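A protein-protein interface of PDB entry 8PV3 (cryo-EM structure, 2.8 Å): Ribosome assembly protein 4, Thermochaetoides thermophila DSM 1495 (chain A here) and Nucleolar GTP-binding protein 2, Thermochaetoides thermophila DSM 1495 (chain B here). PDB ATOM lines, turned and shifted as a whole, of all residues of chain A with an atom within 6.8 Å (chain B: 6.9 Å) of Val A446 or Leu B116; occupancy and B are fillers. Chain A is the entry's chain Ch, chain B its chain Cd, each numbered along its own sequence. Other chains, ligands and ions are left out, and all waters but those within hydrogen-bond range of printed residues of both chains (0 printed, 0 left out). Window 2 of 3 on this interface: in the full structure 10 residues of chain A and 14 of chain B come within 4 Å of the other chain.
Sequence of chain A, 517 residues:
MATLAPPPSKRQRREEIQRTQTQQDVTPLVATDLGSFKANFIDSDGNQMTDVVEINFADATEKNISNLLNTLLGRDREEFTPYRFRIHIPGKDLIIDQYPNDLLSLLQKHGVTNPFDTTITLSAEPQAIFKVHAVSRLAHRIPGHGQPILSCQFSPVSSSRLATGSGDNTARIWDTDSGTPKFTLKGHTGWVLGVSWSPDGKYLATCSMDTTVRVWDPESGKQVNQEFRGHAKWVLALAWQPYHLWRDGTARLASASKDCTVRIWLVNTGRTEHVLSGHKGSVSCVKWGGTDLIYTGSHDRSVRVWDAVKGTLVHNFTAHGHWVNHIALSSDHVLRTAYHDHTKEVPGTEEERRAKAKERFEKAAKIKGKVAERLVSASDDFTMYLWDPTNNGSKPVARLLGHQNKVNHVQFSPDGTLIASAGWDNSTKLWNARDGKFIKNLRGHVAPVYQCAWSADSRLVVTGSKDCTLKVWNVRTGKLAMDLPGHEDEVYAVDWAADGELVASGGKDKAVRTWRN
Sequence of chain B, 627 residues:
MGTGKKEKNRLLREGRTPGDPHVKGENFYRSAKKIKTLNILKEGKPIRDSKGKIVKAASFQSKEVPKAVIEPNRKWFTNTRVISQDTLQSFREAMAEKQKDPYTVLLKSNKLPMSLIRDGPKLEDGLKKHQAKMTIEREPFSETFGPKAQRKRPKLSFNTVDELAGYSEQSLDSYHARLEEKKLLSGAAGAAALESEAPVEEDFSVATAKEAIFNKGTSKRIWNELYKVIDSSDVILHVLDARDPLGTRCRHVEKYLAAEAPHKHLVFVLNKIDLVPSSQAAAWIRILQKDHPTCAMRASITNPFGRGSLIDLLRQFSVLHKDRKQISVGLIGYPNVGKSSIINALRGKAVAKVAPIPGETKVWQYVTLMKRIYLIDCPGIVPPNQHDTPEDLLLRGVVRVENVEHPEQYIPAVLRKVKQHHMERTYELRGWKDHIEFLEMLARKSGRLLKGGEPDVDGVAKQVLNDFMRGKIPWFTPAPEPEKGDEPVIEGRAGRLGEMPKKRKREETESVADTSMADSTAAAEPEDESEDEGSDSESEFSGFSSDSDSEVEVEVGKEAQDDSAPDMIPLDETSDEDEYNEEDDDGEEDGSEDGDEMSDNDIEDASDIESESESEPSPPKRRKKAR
The backbone carbonyl oxygen (O) of Ile B117 is in hydrogen-bond range of the guanidinium group (NH2) of Arg A443 (3.4 Å). O of Gly A444 is in hydrogen-bond range of NE2 of Gln B85. O of Arg A443 is in hydrogen-bond range of NH1 of Arg B92 (3.4 Å). O of Arg B118 lies within hydrogen-bond range of NH2 of Arg A443, 3.5 Å away.
O of Met B114 lies close to NE of Arg B118, 3.5 Å away. OD2 of Asp A467 is in hydrogen-bond range of N of Val A446. The guanidinium group (NE) of Arg B92 lies within hydrogen-bond range of the backbone carbonyl oxygen (O) of Leu B116 (3.3 Å).
NH1 of Arg A443 touches O of Leu B116, at 3.6 Å. Val A446 touches Leu B116. Gln B85 touches Lys A471.
Printed residues of chain B within 4 Å of Val A446: Leu B116 (3.8 Å). Of chain A, only Arg A443 and Val A446 come within 4 Å of Leu B116. Of the printed residues of chain B, Gly A444 touches Gln B85. Printed residues of chain B within 4 Å of Arg A443: Arg B92, Leu B116, Ile B117 and Arg B118. Printed residues of chain A within 4 Å of Arg B92: Arg A443 (3.1 Å). Of the printed residues of chain A, Gln B85 touches Gly A444 and Lys A471. The nearest residue of chain B that does not touch Val A446 is Gln B85 (5.5 Å). The nearest printed residue of chain A that does not touch Arg B92 is Gly A444 (4.9 Å).
Of the 11 printed residues of chain B, 5 touch a printed residue of chain A. Hydrophobic or aromatic side chains of chain B that line the printed part of chain A: Leu B116. Hydrophobic or aromatic side chains of chain A within 4 Å of the printed part of chain B: Val A446. Among the printed residues, no Asp or Glu carboxylate lies within 4 Å of a Lys or Arg side-chain nitrogen of the other chain.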
ATOM      1  N   ASN A 426     -17.434  -6.552  -2.531  1.00  0.00           N
ATOM      2  CA  ASN A 426     -17.356  -5.482  -1.542  1.00  0.00           C
ATOM      3  C   ASN A 426     -18.434  -4.422  -1.739  1.00  0.00           C
ATOM      4  O   ASN A 426     -18.288  -3.301  -1.247  1.00  0.00           O
ATOM      5  CB  ASN A 426     -15.979  -4.805  -1.540  1.00  0.00           C
ATOM      6  CG  ASN A 426     -14.840  -5.795  -1.451  1.00  0.00           C
ATOM      7  OD1 ASN A 426     -14.953  -6.833  -0.814  1.00  0.00           O
ATOM      8  ND2 ASN A 426     -13.727  -5.468  -2.089  1.00  0.00           N
ATOM      9  N   ARG A 443     -20.478   2.085  -2.172  1.00  0.00           N
ATOM     10  CA  ARG A 443     -19.073   1.677  -2.153  1.00  0.00           C
ATOM     11  C   ARG A 443     -18.403   2.201  -0.881  1.00  0.00           C
ATOM     12  O   ARG A 443     -17.816   3.283  -0.870  1.00  0.00           O
ATOM     13  CB  ARG A 443     -18.351   2.170  -3.406  1.00  0.00           C
ATOM     14  CG  ARG A 443     -17.215   1.275  -3.850  1.00  0.00           C
ATOM     15  CD  ARG A 443     -17.055   1.297  -5.362  1.00  0.00           C
ATOM     16  NE  ARG A 443     -16.206   2.381  -5.842  1.00  0.00           N
ATOM     17  CZ  ARG A 443     -14.881   2.391  -5.772  1.00  0.00           C
ATOM     18  NH1 ARG A 443     -14.208   1.396  -5.220  1.00  0.00           N
ATOM     19  NH2 ARG A 443     -14.214   3.421  -6.281  1.00  0.00           N
ATOM     20  N   GLY A 444     -18.493   1.426   0.196  1.00  0.00           N
ATOM     21  CA  GLY A 444     -17.761   1.763   1.399  1.00  0.00           C
ATOM     22  C   GLY A 444     -17.021   0.611   2.047  1.00  0.00           C
ATOM     23  O   GLY A 444     -16.118   0.836   2.858  1.00  0.00           O
ATOM     24  N   HIS A 445     -17.363  -0.621   1.685  1.00  0.00           N
ATOM     25  CA  HIS A 445     -16.822  -1.805   2.342  1.00  0.00           C
ATOM     26  C   HIS A 445     -15.561  -2.263   1.623  1.00  0.00           C
ATOM     27  O   HIS A 445     -15.421  -2.056   0.413  1.00  0.00           O
ATOM     28  CB  HIS A 445     -17.850  -2.936   2.372  1.00  0.00           C
ATOM     29  CG  HIS A 445     -18.889  -2.786   3.440  1.00  0.00           C
ATOM     30  ND1 HIS A 445     -18.583  -2.796   4.783  1.00  0.00           N
ATOM     31  CD2 HIS A 445     -20.233  -2.646   3.363  1.00  0.00           C
ATOM     32  CE1 HIS A 445     -19.693  -2.656   5.487  1.00  0.00           C
ATOM     33  NE2 HIS A 445     -20.708  -2.565   4.648  1.00  0.00           N
ATOM     34  N   VAL A 446     -14.643  -2.878   2.370  1.00  0.00           N
ATOM     35  CA  VAL A 446     -13.377  -3.309   1.785  1.00  0.00           C
ATOM     36  C   VAL A 446     -13.284  -4.828   1.768  1.00  0.00           C
ATOM     37  O   VAL A 446     -12.366  -5.404   1.170  1.00  0.00           O
ATOM     38  CB  VAL A 446     -12.198  -2.672   2.541  1.00  0.00           C
ATOM     39  CG1 VAL A 446     -12.156  -1.179   2.284  1.00  0.00           C
ATOM     40  CG2 VAL A 446     -12.313  -2.949   4.028  1.00  0.00           C
ATOM     41  N   ALA A 447     -14.218  -5.496   2.422  1.00  0.00           N
ATOM     42  CA  ALA A 447     -14.354  -6.941   2.441  1.00  0.00           C
ATOM     43  C   ALA A 447     -15.774  -7.320   2.037  1.00  0.00           C
ATOM     44  O   ALA A 447     -16.680  -6.479   2.069  1.00  0.00           O
ATOM     45  CB  ALA A 447     -14.018  -7.482   3.835  1.00  0.00           C
ATOM     46  N   PRO A 448     -15.999  -8.586   1.574  1.00  0.00           N
ATOM     47  CA  PRO A 448     -17.335  -8.988   1.101  1.00  0.00           C
ATOM     48  C   PRO A 448     -18.481  -8.754   2.071  1.00  0.00           C
ATOM     49  O   PRO A 448     -18.393  -9.090   3.255  1.00  0.00           O
ATOM     50  CB  PRO A 448     -17.158 -10.485   0.838  1.00  0.00           C
ATOM     51  CG  PRO A 448     -15.763 -10.606   0.403  1.00  0.00           C
ATOM     52  CD  PRO A 448     -14.973  -9.549   1.128  1.00  0.00           C
ATOM     53  N   VAL A 449     -19.566  -8.177   1.562  1.00  0.00           N
ATOM     54  CA  VAL A 449     -20.727  -7.825   2.367  1.00  0.00           C
ATOM     55  C   VAL A 449     -21.579  -9.073   2.530  1.00  0.00           C
ATOM     56  O   VAL A 449     -21.981  -9.695   1.541  1.00  0.00           O
ATOM     57  CB  VAL A 449     -21.528  -6.683   1.725  1.00  0.00           C
ATOM     58  CG1 VAL A 449     -22.584  -6.183   2.683  1.00  0.00           C
ATOM     59  CG2 VAL A 449     -20.600  -5.557   1.333  1.00  0.00           C
ATOM     60  N   SER A 465     -20.630  -6.535   6.948  1.00  0.00           N
ATOM     61  CA  SER A 465     -19.665  -7.143   6.047  1.00  0.00           C
ATOM     62  C   SER A 465     -18.611  -7.936   6.804  1.00  0.00           C
ATOM     63  O   SER A 465     -18.614  -8.024   8.034  1.00  0.00           O
ATOM     64  CB  SER A 465     -18.983  -6.084   5.177  1.00  0.00           C
ATOM     65  OG  SER A 465     -17.894  -6.640   4.465  1.00  0.00           O
ATOM     66  N   ASP A 467     -15.494  -7.117   6.855  1.00  0.00           N
ATOM     67  CA  ASP A 467     -14.492  -6.195   7.378  1.00  0.00           C
ATOM     68  C   ASP A 467     -14.799  -5.700   8.784  1.00  0.00           C
ATOM     69  O   ASP A 467     -14.300  -4.635   9.155  1.00  0.00           O
ATOM     70  CB  ASP A 467     -14.316  -4.996   6.436  1.00  0.00           C
ATOM     71  CG  ASP A 467     -15.594  -4.189   6.236  1.00  0.00           C
ATOM     72  OD1 ASP A 467     -16.652  -4.535   6.797  1.00  0.00           O
ATOM     73  OD2 ASP A 467     -15.534  -3.185   5.501  1.00  0.00           O
ATOM     74  N   THR A 469     -17.465  -4.409  10.024  1.00  0.00           N
ATOM     75  CA  THR A 469     -18.209  -3.162  10.108  1.00  0.00           C
ATOM     76  C   THR A 469     -19.647  -3.321   9.632  1.00  0.00           C
ATOM     77  O   THR A 469     -19.969  -4.149   8.761  1.00  0.00           O
ATOM     78  CB  THR A 469     -17.542  -2.042   9.293  1.00  0.00           C
ATOM     79  OG1 THR A 469     -17.683  -2.311   7.893  1.00  0.00           O
ATOM     80  CG2 THR A 469     -16.073  -1.893   9.648  1.00  0.00           C
ATOM     81  N   LYS A 471     -22.634  -0.661   8.043  1.00  0.00           N
ATOM     82  CA  LYS A 471     -22.781   0.646   7.422  1.00  0.00           C
ATOM     83  C   LYS A 471     -24.245   0.925   7.134  1.00  0.00           C
ATOM     84  O   LYS A 471     -24.942   0.090   6.558  1.00  0.00           O
ATOM     85  CB  LYS A 471     -21.964   0.759   6.131  1.00  0.00           C
ATOM     86  CG  LYS A 471     -20.469   0.723   6.350  1.00  0.00           C
ATOM     87  CD  LYS A 471     -19.702   1.256   5.171  1.00  0.00           C
ATOM     88  CE  LYS A 471     -18.239   0.921   5.316  1.00  0.00           C
ATOM     89  NZ  LYS A 471     -17.730   1.241   6.670  1.00  0.00           N
ATOM     90  N   ILE B  83      -6.604   5.814   6.187  1.00  0.00           N
ATOM     91  CA  ILE B  83      -7.378   6.749   5.379  1.00  0.00           C
ATOM     92  C   ILE B  83      -8.844   6.619   5.776  1.00  0.00           C
ATOM     93  O   ILE B  83      -9.301   5.539   6.162  1.00  0.00           O
ATOM     94  CB  ILE B  83      -7.150   6.506   3.866  1.00  0.00           C
ATOM     95  CG1 ILE B  83      -7.722   7.650   3.027  1.00  0.00           C
ATOM     96  CG2 ILE B  83      -7.708   5.162   3.417  1.00  0.00           C
ATOM     97  CD1 ILE B  83      -7.276   7.631   1.592  1.00  0.00           C
ATOM     98  N   GLN B  85     -13.170   7.350   5.265  1.00  0.00           N
ATOM     99  CA  GLN B  85     -14.171   7.145   4.226  1.00  0.00           C
ATOM    100  C   GLN B  85     -14.490   8.442   3.494  1.00  0.00           C
ATOM    101  O   GLN B  85     -14.754   8.429   2.287  1.00  0.00           O
ATOM    102  CB  GLN B  85     -15.438   6.546   4.833  1.00  0.00           C
ATOM    103  CG  GLN B  85     -15.246   5.159   5.422  1.00  0.00           C
ATOM    104  CD  GLN B  85     -15.231   4.071   4.370  1.00  0.00           C
ATOM    105  OE1 GLN B  85     -15.559   4.306   3.209  1.00  0.00           O
ATOM    106  NE2 GLN B  85     -14.853   2.867   4.775  1.00  0.00           N
ATOM    107  N   LEU B  88     -11.657   8.959   1.105  1.00  0.00           N
ATOM    108  CA  LEU B  88     -11.810   8.030  -0.011  1.00  0.00           C
ATOM    109  C   LEU B  88     -12.898   8.485  -0.976  1.00  0.00           C
ATOM    110  O   LEU B  88     -12.724   8.399  -2.194  1.00  0.00           O
ATOM    111  CB  LEU B  88     -12.112   6.625   0.506  1.00  0.00           C
ATOM    112  CG  LEU B  88     -10.898   5.784   0.898  1.00  0.00           C
ATOM    113  CD1 LEU B  88     -11.335   4.488   1.553  1.00  0.00           C
ATOM    114  CD2 LEU B  88     -10.040   5.507  -0.321  1.00  0.00           C
ATOM    115  N   ARG B  92     -12.477   9.521  -4.832  1.00  0.00           N
ATOM    116  CA  ARG B  92     -13.299   8.915  -5.879  1.00  0.00           C
ATOM    117  C   ARG B  92     -13.926   9.977  -6.772  1.00  0.00           C
ATOM    118  O   ARG B  92     -13.941   9.839  -8.001  1.00  0.00           O
ATOM    119  CB  ARG B  92     -14.392   8.043  -5.262  1.00  0.00           C
ATOM    120  CG  ARG B  92     -13.910   6.748  -4.648  1.00  0.00           C
ATOM    121  CD  ARG B  92     -15.077   5.888  -4.203  1.00  0.00           C
ATOM    122  NE  ARG B  92     -14.632   4.712  -3.466  1.00  0.00           N
ATOM    123  CZ  ARG B  92     -14.735   4.568  -2.153  1.00  0.00           C
ATOM    124  NH1 ARG B  92     -15.293   5.499  -1.398  1.00  0.00           N
ATOM    125  NH2 ARG B  92     -14.268   3.462  -1.582  1.00  0.00           N
ATOM    126  N   PRO B 113      -4.037   4.579  -1.824  1.00  0.00           N
ATOM    127  CA  PRO B 113      -4.553   3.216  -2.072  1.00  0.00           C
ATOM    128  C   PRO B 113      -5.451   3.210  -3.305  1.00  0.00           C
ATOM    129  O   PRO B 113      -6.676   3.304  -3.244  1.00  0.00           O
ATOM    130  CB  PRO B 113      -5.318   2.907  -0.784  1.00  0.00           C
ATOM    131  CG  PRO B 113      -5.750   4.235  -0.277  1.00  0.00           C
ATOM    132  CD  PRO B 113      -4.682   5.211  -0.660  1.00  0.00           C
ATOM    133  N   MET B 114      -4.813   3.096  -4.472  1.00  0.00           N
ATOM    134  CA  MET B 114      -5.496   3.387  -5.728  1.00  0.00           C
ATOM    135  C   MET B 114      -6.508   2.308  -6.094  1.00  0.00           C
ATOM    136  O   MET B 114      -7.401   2.550  -6.913  1.00  0.00           O
ATOM    137  CB  MET B 114      -4.468   3.561  -6.843  1.00  0.00           C
ATOM    138  CG  MET B 114      -3.883   4.964  -6.922  1.00  0.00           C
ATOM    139  SD  MET B 114      -5.103   6.291  -6.958  1.00  0.00           S
ATOM    140  CE  MET B 114      -5.568   6.289  -8.684  1.00  0.00           C
ATOM    141  N   SER B 115      -6.392   1.120  -5.497  1.00  0.00           N
ATOM    142  CA  SER B 115      -7.385   0.075  -5.719  1.00  0.00           C
ATOM    143  C   SER B 115      -8.725   0.412  -5.080  1.00  0.00           C
ATOM    144  O   SER B 115      -9.759  -0.086  -5.537  1.00  0.00           O
ATOM    145  CB  SER B 115      -6.879  -1.259  -5.181  1.00  0.00           C
ATOM    146  OG  SER B 115      -6.761  -1.221  -3.771  1.00  0.00           O
ATOM    147  N   LEU B 116      -8.729   1.231  -4.031  1.00  0.00           N
ATOM    148  CA  LEU B 116      -9.953   1.691  -3.394  1.00  0.00           C
ATOM    149  C   LEU B 116     -10.506   2.957  -4.031  1.00  0.00           C
ATOM    150  O   LEU B 116     -11.631   3.352  -3.715  1.00  0.00           O
ATOM    151  CB  LEU B 116      -9.716   1.936  -1.901  1.00  0.00           C
ATOM    152  CG  LEU B 116      -9.156   0.792  -1.056  1.00  0.00           C
ATOM    153  CD1 LEU B 116      -8.650   1.319   0.275  1.00  0.00           C
ATOM    154  CD2 LEU B 116     -10.216  -0.269  -0.840  1.00  0.00           C
ATOM    155  N   ILE B 117      -9.748   3.597  -4.924  1.00  0.00           N
ATOM    156  CA  ILE B 117     -10.135   4.863  -5.526  1.00  0.00           C
ATOM    157  C   ILE B 117     -10.575   4.694  -6.974  1.00  0.00           C
ATOM    158  O   ILE B 117     -11.593   5.265  -7.386  1.00  0.00           O
ATOM    159  CB  ILE B 117      -8.988   5.895  -5.421  1.00  0.00           C
ATOM    160  CG1 ILE B 117      -8.615   6.119  -3.957  1.00  0.00           C
ATOM    161  CG2 ILE B 117      -9.377   7.218  -6.057  1.00  0.00           C
ATOM    162  CD1 ILE B 117      -7.410   6.995  -3.767  1.00  0.00           C
ATOM    163  N   ARG B 118      -9.839   3.906  -7.759  1.00  0.00           N
ATOM    164  CA  ARG B 118     -10.167   3.717  -9.168  1.00  0.00           C
ATOM    165  C   ARG B 118     -11.498   2.993  -9.334  1.00  0.00           C
ATOM    166  O   ARG B 118     -11.884   2.154  -8.518  1.00  0.00           O
ATOM    167  CB  ARG B 118      -9.064   2.930  -9.876  1.00  0.00           C
ATOM    168  CG  ARG B 118      -7.791   3.716 -10.140  1.00  0.00           C
ATOM    169  CD  ARG B 118      -6.777   2.882 -10.911  1.00  0.00           C
ATOM    170  NE  ARG B 118      -6.193   1.830 -10.089  1.00  0.00           N
ATOM    171  CZ  ARG B 118      -6.455   0.537 -10.227  1.00  0.00           C
ATOM    172  NH1 ARG B 118      -7.295   0.096 -11.149  1.00  0.00           N
ATOM    173  NH2 ARG B 118      -5.866  -0.335  -9.413  1.00  0.00           N
ATOM    174  N   ASP B 119     -12.208   3.343 -10.404  1.00  0.00           N
ATOM    175  CA  ASP B 119     -13.464   2.689 -10.731  1.00  0.00           C
ATOM    176  C   ASP B 119     -13.217   1.236 -11.127  1.00  0.00           C
ATOM    177  O   ASP B 119     -12.186   0.886 -11.707  1.00  0.00           O
ATOM    178  CB  ASP B 119     -14.176   3.437 -11.859  1.00  0.00           C
ATOM    179  CG  ASP B 119     -15.671   3.181 -11.878  1.00  0.00           C
ATOM    180  OD1 ASP B 119     -16.439   4.118 -11.575  1.00  0.00           O
ATOM    181  OD2 ASP B 119     -16.077   2.046 -12.205  1.00  0.00           O
